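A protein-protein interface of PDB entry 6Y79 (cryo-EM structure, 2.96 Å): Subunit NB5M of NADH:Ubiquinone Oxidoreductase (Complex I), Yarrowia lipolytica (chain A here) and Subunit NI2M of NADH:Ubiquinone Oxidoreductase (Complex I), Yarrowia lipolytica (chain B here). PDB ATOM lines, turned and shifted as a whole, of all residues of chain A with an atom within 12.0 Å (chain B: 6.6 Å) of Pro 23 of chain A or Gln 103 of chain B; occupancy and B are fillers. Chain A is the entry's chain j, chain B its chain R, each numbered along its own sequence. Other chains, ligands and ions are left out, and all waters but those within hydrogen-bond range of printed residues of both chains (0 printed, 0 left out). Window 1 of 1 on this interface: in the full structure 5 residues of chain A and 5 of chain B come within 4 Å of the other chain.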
ATOM      1  N   GLY A  19     -15.545 -26.480 -30.146  1.00  0.00           N
ATOM      2  CA  GLY A  19     -14.789 -26.358 -28.924  1.00  0.00           C
ATOM      3  C   GLY A  19     -13.705 -25.305 -28.967  1.00  0.00           C
ATOM      4  O   GLY A  19     -13.864 -24.235 -29.565  1.00  0.00           O
ATOM      5  N   TRP A  20     -12.588 -25.621 -28.330  1.00  0.00           N
ATOM      6  CA  TRP A  20     -11.515 -24.682 -28.060  1.00  0.00           C
ATOM      7  C   TRP A  20     -10.290 -25.098 -28.851  1.00  0.00           C
ATOM      8  O   TRP A  20      -9.947 -26.280 -28.895  1.00  0.00           O
ATOM      9  CB  TRP A  20     -11.212 -24.682 -26.566  1.00  0.00           C
ATOM     10  CG  TRP A  20     -10.204 -23.712 -26.059  1.00  0.00           C
ATOM     11  CD1 TRP A  20     -10.290 -22.358 -26.066  1.00  0.00           C
ATOM     12  CD2 TRP A  20      -8.978 -24.035 -25.402  1.00  0.00           C
ATOM     13  NE1 TRP A  20      -9.181 -21.813 -25.473  1.00  0.00           N
ATOM     14  CE2 TRP A  20      -8.359 -22.825 -25.057  1.00  0.00           C
ATOM     15  CE3 TRP A  20      -8.339 -25.234 -25.084  1.00  0.00           C
ATOM     16  CZ2 TRP A  20      -7.132 -22.777 -24.409  1.00  0.00           C
ATOM     17  CZ3 TRP A  20      -7.128 -25.183 -24.447  1.00  0.00           C
ATOM     18  CH2 TRP A  20      -6.534 -23.968 -24.112  1.00  0.00           C
ATOM     19  N   ASP A  21      -9.639 -24.135 -29.490  1.00  0.00           N
ATOM     20  CA  ASP A  21      -8.374 -24.432 -30.151  1.00  0.00           C
ATOM     21  C   ASP A  21      -7.267 -24.321 -29.118  1.00  0.00           C
ATOM     22  O   ASP A  21      -6.900 -23.221 -28.698  1.00  0.00           O
ATOM     23  CB  ASP A  21      -8.119 -23.508 -31.331  1.00  0.00           C
ATOM     24  CG  ASP A  21      -7.146 -24.116 -32.320  1.00  0.00           C
ATOM     25  OD1 ASP A  21      -7.325 -25.307 -32.644  1.00  0.00           O
ATOM     26  OD2 ASP A  21      -6.201 -23.429 -32.756  1.00  0.00           O
ATOM     27  N   ALA A  22      -6.749 -25.466 -28.698  1.00  0.00           N
ATOM     28  CA  ALA A  22      -5.652 -25.499 -27.743  1.00  0.00           C
ATOM     29  C   ALA A  22      -4.396 -24.957 -28.404  1.00  0.00           C
ATOM     30  O   ALA A  22      -4.083 -25.361 -29.529  1.00  0.00           O
ATOM     31  CB  ALA A  22      -5.421 -26.919 -27.244  1.00  0.00           C
ATOM     32  N   PRO A  23      -3.688 -24.017 -27.784  1.00  0.00           N
ATOM     33  CA  PRO A  23      -2.436 -23.533 -28.369  1.00  0.00           C
ATOM     34  C   PRO A  23      -1.366 -24.612 -28.370  1.00  0.00           C
ATOM     35  O   PRO A  23      -1.399 -25.553 -27.574  1.00  0.00           O
ATOM     36  CB  PRO A  23      -2.050 -22.362 -27.462  1.00  0.00           C
ATOM     37  CG  PRO A  23      -2.793 -22.594 -26.196  1.00  0.00           C
ATOM     38  CD  PRO A  23      -4.064 -23.259 -26.583  1.00  0.00           C
ATOM     39  N   HIS A  24      -0.413 -24.462 -29.288  1.00  0.00           N
ATOM     40  CA  HIS A  24       0.527 -25.531 -29.611  1.00  0.00           C
ATOM     41  C   HIS A  24       1.545 -25.697 -28.495  1.00  0.00           C
ATOM     42  O   HIS A  24       2.402 -24.833 -28.286  1.00  0.00           O
ATOM     43  CB  HIS A  24       1.218 -25.237 -30.936  1.00  0.00           C
ATOM     44  CG  HIS A  24       0.284 -25.217 -32.101  1.00  0.00           C
ATOM     45  ND1 HIS A  24      -0.375 -24.077 -32.506  1.00  0.00           N
ATOM     46  CD2 HIS A  24      -0.120 -26.202 -32.937  1.00  0.00           C
ATOM     47  CE1 HIS A  24      -1.137 -24.357 -33.547  1.00  0.00           C
ATOM     48  NE2 HIS A  24      -1.001 -25.640 -33.828  1.00  0.00           N
ATOM     49  N   ALA A  25       1.452 -26.814 -27.783  1.00  0.00           N
ATOM     50  CA  ALA A  25       2.374 -27.133 -26.708  1.00  0.00           C
ATOM     51  C   ALA A  25       3.649 -27.785 -27.200  1.00  0.00           C
ATOM     52  O   ALA A  25       4.568 -27.985 -26.406  1.00  0.00           O
ATOM     53  CB  ALA A  25       1.701 -28.060 -25.709  1.00  0.00           C
ATOM     54  N   LEU A  26       3.731 -28.119 -28.479  1.00  0.00           N
ATOM     55  CA  LEU A  26       4.855 -28.891 -28.974  1.00  0.00           C
ATOM     56  C   LEU A  26       5.289 -28.365 -30.326  1.00  0.00           C
ATOM     57  O   LEU A  26       4.478 -28.272 -31.249  1.00  0.00           O
ATOM     58  CB  LEU A  26       4.497 -30.367 -29.098  1.00  0.00           C
ATOM     59  CG  LEU A  26       5.634 -31.201 -29.680  1.00  0.00           C
ATOM     60  CD1 LEU A  26       6.538 -31.723 -28.583  1.00  0.00           C
ATOM     61  CD2 LEU A  26       5.093 -32.318 -30.519  1.00  0.00           C
ATOM     62  N   HIS A  27       6.570 -28.032 -30.439  1.00  0.00           N
ATOM     63  CA  HIS A  27       7.161 -27.673 -31.719  1.00  0.00           C
ATOM     64  C   HIS A  27       7.481 -28.950 -32.472  1.00  0.00           C
ATOM     65  O   HIS A  27       8.272 -29.765 -32.001  1.00  0.00           O
ATOM     66  CB  HIS A  27       8.417 -26.836 -31.510  1.00  0.00           C
ATOM     67  CG  HIS A  27       8.226 -25.697 -30.564  1.00  0.00           C
ATOM     68  ND1 HIS A  27       8.350 -25.835 -29.199  1.00  0.00           N
ATOM     69  CD2 HIS A  27       7.897 -24.404 -30.785  1.00  0.00           C
ATOM     70  CE1 HIS A  27       8.114 -24.673 -28.621  1.00  0.00           C
ATOM     71  NE2 HIS A  27       7.837 -23.787 -29.560  1.00  0.00           N
ATOM     72  N   ASN A  28       6.849 -29.127 -33.627  1.00  0.00           N
ATOM     73  CA  ASN A  28       7.089 -30.273 -34.482  1.00  0.00           C
ATOM     74  C   ASN A  28       8.532 -30.273 -34.949  1.00  0.00           C
ATOM     75  O   ASN A  28       9.158 -29.224 -35.148  1.00  0.00           O
ATOM     76  CB  ASN A  28       6.196 -30.256 -35.706  1.00  0.00           C
ATOM     77  CG  ASN A  28       4.720 -30.272 -35.355  1.00  0.00           C
ATOM     78  OD1 ASN A  28       4.023 -29.269 -35.526  1.00  0.00           O
ATOM     79  ND2 ASN A  28       4.220 -31.419 -34.915  1.00  0.00           N
ATOM     80  N   ILE B 101       2.769 -21.784 -18.028  1.00  0.00           N
ATOM     81  CA  ILE B 101       2.098 -23.035 -18.355  1.00  0.00           C
ATOM     82  C   ILE B 101       1.268 -22.862 -19.619  1.00  0.00           C
ATOM     83  O   ILE B 101       0.362 -22.024 -19.671  1.00  0.00           O
ATOM     84  CB  ILE B 101       1.224 -23.500 -17.187  1.00  0.00           C
ATOM     85  CG1 ILE B 101       2.086 -23.824 -15.976  1.00  0.00           C
ATOM     86  CG2 ILE B 101       0.425 -24.695 -17.585  1.00  0.00           C
ATOM     87  CD1 ILE B 101       1.287 -24.085 -14.734  1.00  0.00           C
ATOM     88  N   MET B 102       1.575 -23.654 -20.641  1.00  0.00           N
ATOM     89  CA  MET B 102       0.721 -23.764 -21.813  1.00  0.00           C
ATOM     90  C   MET B 102      -0.452 -24.669 -21.481  1.00  0.00           C
ATOM     91  O   MET B 102      -0.303 -25.646 -20.748  1.00  0.00           O
ATOM     92  CB  MET B 102       1.516 -24.327 -22.989  1.00  0.00           C
ATOM     93  CG  MET B 102       0.779 -24.415 -24.296  1.00  0.00           C
ATOM     94  SD  MET B 102       0.680 -22.812 -25.077  1.00  0.00           S
ATOM     95  CE  MET B 102       2.414 -22.507 -25.365  1.00  0.00           C
ATOM     96  N   GLN B 103      -1.628 -24.344 -21.998  1.00  0.00           N
ATOM     97  CA  GLN B 103      -2.819 -25.088 -21.630  1.00  0.00           C
ATOM     98  C   GLN B 103      -3.423 -25.784 -22.839  1.00  0.00           C
ATOM     99  O   GLN B 103      -3.390 -25.272 -23.960  1.00  0.00           O
ATOM    100  CB  GLN B 103      -3.826 -24.179 -20.945  1.00  0.00           C
ATOM    101  CG  GLN B 103      -3.363 -23.841 -19.552  1.00  0.00           C
ATOM    102  CD  GLN B 103      -4.341 -23.012 -18.788  1.00  0.00           C
ATOM    103  OE1 GLN B 103      -5.412 -22.675 -19.292  1.00  0.00           O
ATOM    104  NE2 GLN B 103      -3.993 -22.678 -17.554  1.00  0.00           N
ATOM    105  N   HIS B 104      -3.962 -26.973 -22.590  1.00  0.00           N
ATOM    106  CA  HIS B 104      -4.386 -27.889 -23.631  1.00  0.00           C
ATOM    107  C   HIS B 104      -5.870 -28.213 -23.581  1.00  0.00           C
ATOM    108  O   HIS B 104      -6.381 -28.825 -24.523  1.00  0.00           O
ATOM    109  CB  HIS B 104      -3.593 -29.201 -23.527  1.00  0.00           C
ATOM    110  CG  HIS B 104      -3.876 -29.960 -22.270  1.00  0.00           C
ATOM    111  ND1 HIS B 104      -3.318 -29.622 -21.058  1.00  0.00           N
ATOM    112  CD2 HIS B 104      -4.689 -31.013 -22.029  1.00  0.00           C
ATOM    113  CE1 HIS B 104      -3.766 -30.442 -20.127  1.00  0.00           C
ATOM    114  NE2 HIS B 104      -4.602 -31.294 -20.689  1.00  0.00           N
ATOM    115  N   ASN B 105      -6.575 -27.821 -22.531  1.00  0.00           N
ATOM    116  CA  ASN B 105      -7.969 -28.186 -22.360  1.00  0.00           C
ATOM    117  C   ASN B 105      -8.774 -26.963 -21.948  1.00  0.00           C
ATOM    118  O   ASN B 105      -8.300 -26.124 -21.181  1.00  0.00           O
ATOM    119  CB  ASN B 105      -8.105 -29.301 -21.320  1.00  0.00           C
ATOM    120  CG  ASN B 105      -9.461 -29.952 -21.340  1.00  0.00           C
ATOM    121  OD1 ASN B 105     -10.256 -29.744 -22.256  1.00  0.00           O
ATOM    122  ND2 ASN B 105      -9.731 -30.761 -20.334  1.00  0.00           N
ATOM    123  N   GLU B 108     -10.387 -28.205 -17.954  1.00  0.00           N
ATOM    124  CA  GLU B 108      -9.573 -28.754 -16.890  1.00  0.00           C
ATOM    125  C   GLU B 108      -8.158 -28.215 -17.026  1.00  0.00           C
ATOM    126  O   GLU B 108      -7.702 -27.969 -18.144  1.00  0.00           O
ATOM    127  CB  GLU B 108      -9.583 -30.279 -17.010  1.00  0.00           C
ATOM    128  CG  GLU B 108      -8.538 -31.070 -16.273  1.00  0.00           C
ATOM    129  CD  GLU B 108      -8.302 -32.416 -16.936  1.00  0.00           C
ATOM    130  OE1 GLU B 108      -8.029 -32.437 -18.153  1.00  0.00           O
ATOM    131  OE2 GLU B 108      -8.416 -33.455 -16.261  1.00  0.00           O
ATOM    132  N   PRO B 109      -7.470 -27.935 -15.918  1.00  0.00           N
ATOM    133  CA  PRO B 109      -6.052 -27.625 -16.099  1.00  0.00           C
ATOM    134  C   PRO B 109      -5.264 -28.853 -16.514  1.00  0.00           C
ATOM    135  O   PRO B 109      -5.099 -29.022 -17.719  1.00  0.00           O
ATOM    136  CB  PRO B 109      -5.629 -27.141 -14.719  1.00  0.00           C
ATOM    137  CG  PRO B 109      -6.863 -26.632 -14.097  1.00  0.00           C
ATOM    138  CD  PRO B 109      -7.942 -27.559 -14.579  1.00  0.00           C
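OE1 of Glu 108 of chain B sits at hydrogen-bond distance from ND2 of Asn 105 of chain B.
Gln 103 of chain B touches Trp 20 of chain A (O to CH2, 3.4 Å).
Trp 20 of chain A touches His 104 of chain B.
Asn 105 of chain B touches Trp 20 of chain A (N to CZ3, 3.3 Å).
Ala 22 of chain A touches His 104 of chain B.
Pro 23 of chain A touches Met 102 of chain B.
Pro 23 of chain A touches Gln 103 of chain B (CD to O, 3.4 Å).
His 24 of chain A touches Met 102 of chain B.
Ala 25 of chain A touches Met 102 of chain B.
Pro 23 of chain A touches just these residues of chain B: Met 102 and Gln 103.
Of the printed residues of chain A, Gln 103 of chain B touches Trp 20 and Pro 23.
No residue of chain A comes within 4 Å of Ile 101 of chain B.
Of chain A, only Pro 23 (3.7 Å), His 24 (3.7 Å) and Ala 25 (3.97 Å) come within 4 Å of Met 102 of chain B.
No residue of chain A comes within 4 Å of Pro 109 of chain B.
Of the printed residues of chain B, His 24 of chain A touches Met 102 (3.7 Å).
Printed residues of chain B within 4 Å of Ala 25 of chain A: Met 102 (3.97 Å).
Of the printed residues of chain A, Asn 105 of chain B touches Trp 20 (3.3 Å).
Of the printed residues of chain B, Trp 20 of chain A touches Gln 103 (3.4 Å), His 104 (3.4 Å) and Asn 105 (3.3 Å).
His 27 of chain A touches none of the printed residues of chain B.
The nearest residue of chain B that does not touch Pro 23 of chain A is His 104 of chain B (5.5 Å).
The nearest residue of chain A that does not touch Gln 103 of chain B is Ala 22 of chain A (4.2 Å).
Of the 10 printed residues of chain A, 5 touch a printed residue of chain B.
Hydrophobic or aromatic side chains of chain A within 4 Å of the printed part of chain B: Trp 20, Ala 22 and Pro 23.
Of the 7 printed residues of chain B, 4 touch a printed residue of chain A.
Among the printed residues, no Asp or Glu carboxylate lies within 4 Å of a Lys or Arg side-chain nitrogen of the other chain.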
